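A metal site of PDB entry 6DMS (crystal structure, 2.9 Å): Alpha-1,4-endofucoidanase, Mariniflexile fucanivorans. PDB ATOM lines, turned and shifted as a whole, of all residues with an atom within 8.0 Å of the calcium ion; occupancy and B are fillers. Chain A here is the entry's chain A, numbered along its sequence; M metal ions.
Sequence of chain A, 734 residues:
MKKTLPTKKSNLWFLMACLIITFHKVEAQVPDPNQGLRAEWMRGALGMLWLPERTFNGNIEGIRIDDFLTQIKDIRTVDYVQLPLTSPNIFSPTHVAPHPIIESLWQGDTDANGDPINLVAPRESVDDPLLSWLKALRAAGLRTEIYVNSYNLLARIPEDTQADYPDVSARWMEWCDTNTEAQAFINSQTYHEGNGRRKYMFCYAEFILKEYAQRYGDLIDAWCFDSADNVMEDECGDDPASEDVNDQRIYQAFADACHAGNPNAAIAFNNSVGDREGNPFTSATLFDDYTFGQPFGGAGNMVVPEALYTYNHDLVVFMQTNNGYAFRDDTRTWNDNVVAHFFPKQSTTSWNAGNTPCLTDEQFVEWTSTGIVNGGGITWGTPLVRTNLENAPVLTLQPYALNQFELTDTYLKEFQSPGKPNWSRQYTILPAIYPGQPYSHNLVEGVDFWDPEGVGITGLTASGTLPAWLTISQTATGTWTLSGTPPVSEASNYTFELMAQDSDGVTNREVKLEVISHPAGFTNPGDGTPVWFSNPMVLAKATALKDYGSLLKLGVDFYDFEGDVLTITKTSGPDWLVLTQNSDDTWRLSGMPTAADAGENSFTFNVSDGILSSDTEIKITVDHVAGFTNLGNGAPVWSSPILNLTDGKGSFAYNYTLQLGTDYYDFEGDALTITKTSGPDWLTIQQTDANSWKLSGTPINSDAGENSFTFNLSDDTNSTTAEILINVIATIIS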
ATOM      1  N   ALA A 326     -12.382 -24.229  14.858  1.00  0.00           N
ATOM      2  CA  ALA A 326     -13.617 -23.435  14.886  1.00  0.00           C
ATOM      3  C   ALA A 326     -13.736 -22.445  16.050  1.00  0.00           C
ATOM      4  O   ALA A 326     -14.246 -21.339  15.869  1.00  0.00           O
ATOM      5  CB  ALA A 326     -14.825 -24.358  14.850  1.00  0.00           C
ATOM      6  N   PHE A 327     -13.277 -22.854  17.241  1.00  0.00           N
ATOM      7  CA  PHE A 327     -13.524 -22.079  18.465  1.00  0.00           C
ATOM      8  C   PHE A 327     -12.258 -21.741  19.264  1.00  0.00           C
ATOM      9  O   PHE A 327     -12.125 -22.125  20.438  1.00  0.00           O
ATOM     10  CB  PHE A 327     -14.582 -22.777  19.345  1.00  0.00           C
ATOM     11  CG  PHE A 327     -15.810 -23.188  18.599  1.00  0.00           C
ATOM     12  CD1 PHE A 327     -16.733 -22.236  18.145  1.00  0.00           C
ATOM     13  CD2 PHE A 327     -16.058 -24.534  18.334  1.00  0.00           C
ATOM     14  CE1 PHE A 327     -17.868 -22.623  17.445  1.00  0.00           C
ATOM     15  CE2 PHE A 327     -17.187 -24.934  17.641  1.00  0.00           C
ATOM     16  CZ  PHE A 327     -18.097 -23.976  17.187  1.00  0.00           C
ATOM     17  N   ARG A 328     -11.335 -21.017  18.639  1.00  0.00           N
ATOM     18  CA  ARG A 328     -10.169 -20.474  19.338  1.00  0.00           C
ATOM     19  C   ARG A 328     -10.300 -18.970  19.593  1.00  0.00           C
ATOM     20  O   ARG A 328      -9.334 -18.302  19.991  1.00  0.00           O
ATOM     21  CB  ARG A 328      -8.868 -20.844  18.613  1.00  0.00           C
ATOM     22  CG  ARG A 328      -8.457 -22.292  18.815  1.00  0.00           C
ATOM     23  CD  ARG A 328      -7.025 -22.534  18.392  1.00  0.00           C
ATOM     24  NE  ARG A 328      -6.692 -23.955  18.450  1.00  0.00           N
ATOM     25  CZ  ARG A 328      -5.512 -24.492  18.136  1.00  0.00           C
ATOM     26  NH1 ARG A 328      -4.499 -23.725  17.746  1.00  0.00           N
ATOM     27  NH2 ARG A 328      -5.334 -25.801  18.232  1.00  0.00           N
ATOM     28  N   ASP A 329     -11.505 -18.455  19.359  1.00  0.00           N
ATOM     29  CA  ASP A 329     -11.834 -17.044  19.548  1.00  0.00           C
ATOM     30  C   ASP A 329     -12.533 -16.761  20.887  1.00  0.00           C
ATOM     31  O   ASP A 329     -12.329 -15.697  21.481  1.00  0.00           O
ATOM     32  CB  ASP A 329     -12.684 -16.514  18.380  1.00  0.00           C
ATOM     33  CG  ASP A 329     -13.955 -17.346  18.146  1.00  0.00           C
ATOM     34  OD1 ASP A 329     -13.863 -18.580  17.978  1.00  0.00           O
ATOM     35  OD2 ASP A 329     -15.050 -16.739  18.100  1.00  0.00           O
ATOM     36  N   ASP A 330     -13.332 -17.720  21.349  1.00  0.00           N
ATOM     37  CA  ASP A 330     -14.132 -17.577  22.571  1.00  0.00           C
ATOM     38  C   ASP A 330     -13.316 -17.695  23.872  1.00  0.00           C
ATOM     39  O   ASP A 330     -12.103 -17.904  23.837  1.00  0.00           O
ATOM     40  CB  ASP A 330     -15.323 -18.563  22.551  1.00  0.00           C
ATOM     41  CG  ASP A 330     -14.894 -20.030  22.670  1.00  0.00           C
ATOM     42  OD1 ASP A 330     -13.727 -20.377  22.387  1.00  0.00           O
ATOM     43  OD2 ASP A 330     -15.755 -20.856  23.040  1.00  0.00           O
ATOM     44  N   THR A 331     -14.002 -17.555  25.004  1.00  0.00           N
ATOM     45  CA  THR A 331     -13.386 -17.568  26.334  1.00  0.00           C
ATOM     46  C   THR A 331     -13.376 -18.957  27.000  1.00  0.00           C
ATOM     47  O   THR A 331     -13.246 -19.077  28.219  1.00  0.00           O
ATOM     48  CB  THR A 331     -14.051 -16.526  27.272  1.00  0.00           C
ATOM     49  OG1 THR A 331     -15.469 -16.732  27.291  1.00  0.00           O
ATOM     50  CG2 THR A 331     -13.745 -15.101  26.819  1.00  0.00           C
ATOM     51  N   ARG A 332     -13.500 -20.004  26.182  1.00  0.00           N
ATOM     52  CA  ARG A 332     -13.503 -21.396  26.661  1.00  0.00           C
ATOM     53  C   ARG A 332     -12.223 -22.125  26.287  1.00  0.00           C
ATOM     54  O   ARG A 332     -11.684 -21.924  25.196  1.00  0.00           O
ATOM     55  CB  ARG A 332     -14.714 -22.160  26.112  1.00  0.00           C
ATOM     56  CG  ARG A 332     -16.045 -21.746  26.729  1.00  0.00           C
ATOM     57  CD  ARG A 332     -17.198 -22.526  26.128  1.00  0.00           C
ATOM     58  NE  ARG A 332     -18.485 -22.014  26.589  1.00  0.00           N
ATOM     59  CZ  ARG A 332     -19.671 -22.537  26.290  1.00  0.00           C
ATOM     60  NH1 ARG A 332     -19.779 -23.615  25.518  1.00  0.00           N
ATOM     61  NH2 ARG A 332     -20.774 -21.966  26.774  1.00  0.00           N
ATOM     62  N   THR A 333     -11.747 -22.973  27.195  1.00  0.00           N
ATOM     63  CA  THR A 333     -10.475 -23.687  27.036  1.00  0.00           C
ATOM     64  C   THR A 333     -10.595 -25.077  26.382  1.00  0.00           C
ATOM     65  O   THR A 333      -9.722 -25.483  25.612  1.00  0.00           O
ATOM     66  CB  THR A 333      -9.682 -23.763  28.376  1.00  0.00           C
ATOM     67  OG1 THR A 333      -8.551 -24.633  28.227  1.00  0.00           O
ATOM     68  CG2 THR A 333     -10.564 -24.252  29.544  1.00  0.00           C
ATOM     69  N   TRP A 334     -11.687 -25.767  26.674  1.00  0.00           N
ATOM     70  CA  TRP A 334     -11.879 -27.174  26.298  1.00  0.00           C
ATOM     71  C   TRP A 334     -12.205 -27.438  24.813  1.00  0.00           C
ATOM     72  O   TRP A 334     -11.990 -28.555  24.330  1.00  0.00           O
ATOM     73  CB  TRP A 334     -12.942 -27.834  27.196  1.00  0.00           C
ATOM     74  CG  TRP A 334     -14.243 -27.080  27.278  1.00  0.00           C
ATOM     75  CD1 TRP A 334     -14.573 -26.113  28.194  1.00  0.00           C
ATOM     76  CD2 TRP A 334     -15.383 -27.230  26.422  1.00  0.00           C
ATOM     77  NE1 TRP A 334     -15.849 -25.646  27.955  1.00  0.00           N
ATOM     78  CE2 TRP A 334     -16.370 -26.318  26.880  1.00  0.00           C
ATOM     79  CE3 TRP A 334     -15.672 -28.038  25.313  1.00  0.00           C
ATOM     80  CZ2 TRP A 334     -17.630 -26.196  26.257  1.00  0.00           C
ATOM     81  CZ3 TRP A 334     -16.925 -27.916  24.696  1.00  0.00           C
ATOM     82  CH2 TRP A 334     -17.888 -27.002  25.174  1.00  0.00           C
ATOM     83  N   ASN A 335     -12.696 -26.425  24.115  1.00  0.00           N
ATOM     84  CA  ASN A 335     -13.093 -26.540  22.703  1.00  0.00           C
ATOM     85  C   ASN A 335     -12.008 -26.118  21.688  1.00  0.00           C
ATOM     86  O   ASN A 335     -12.291 -25.966  20.494  1.00  0.00           O
ATOM     87  CB  ASN A 335     -14.415 -25.789  22.433  1.00  0.00           C
ATOM     88  CG  ASN A 335     -14.363 -24.315  22.847  1.00  0.00           C
ATOM     89  OD1 ASN A 335     -13.299 -23.694  22.926  1.00  0.00           O
ATOM     90  ND2 ASN A 335     -15.540 -23.751  23.094  1.00  0.00           N
ATOM     91  N   ASP A 336     -10.773 -25.964  22.177  1.00  0.00           N
ATOM     92  CA  ASP A 336      -9.657 -25.435  21.384  1.00  0.00           C
ATOM     93  C   ASP A 336      -9.134 -26.357  20.277  1.00  0.00           C
ATOM     94  O   ASP A 336      -8.395 -25.902  19.395  1.00  0.00           O
ATOM     95  CB  ASP A 336      -8.509 -25.012  22.302  1.00  0.00           C
ATOM     96  CG  ASP A 336      -8.709 -23.622  22.902  1.00  0.00           C
ATOM     97  OD1 ASP A 336      -9.788 -23.015  22.711  1.00  0.00           O
ATOM     98  OD2 ASP A 336      -7.772 -23.146  23.569  1.00  0.00           O
ATOM     99  N   ASN A 337      -9.520 -27.628  20.312  1.00  0.00           N
ATOM    100  CA  ASN A 337      -9.089 -28.604  19.305  1.00  0.00           C
ATOM    101  C   ASN A 337     -10.179 -28.984  18.298  1.00  0.00           C
ATOM    102  O   ASN A 337      -9.923 -29.750  17.359  1.00  0.00           O
ATOM    103  CB  ASN A 337      -8.509 -29.860  19.980  1.00  0.00           C
ATOM    104  CG  ASN A 337      -7.199 -29.593  20.698  1.00  0.00           C
ATOM    105  OD1 ASN A 337      -7.084 -29.850  21.900  1.00  0.00           O
ATOM    106  ND2 ASN A 337      -6.212 -29.078  19.967  1.00  0.00           N
HETATM  107 CA    CA M   1     -11.662 -21.583  22.754  1.00  0.00          CA
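O of Asp 336 lies within hydrogen-bond range of NE of Arg 328, at 2.8 Å.
Residues that only touch the calcium ion: Arg 328.
Six residues have an atom within 4 Å of the calcium ion: Phe 327, Arg 328, Asp 330, Arg 332, Asn 335 and Asp 336.
The nearest printed residue that does not touch the calcium ion is Asp 329 (4.6 Å).
The calcium ion is bound by the side-chain carboxylate of Asp 336 (2.4 Å), the side-chain carboxylate of Asp 330 (2.4 Å), the backbone carbonyl oxygen of Phe 327 (2.4 Å), the backbone carbonyl oxygen of Arg 332 (2.5 Å) and the side-chain amide oxygen of Asn 335 (2.7 Å).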
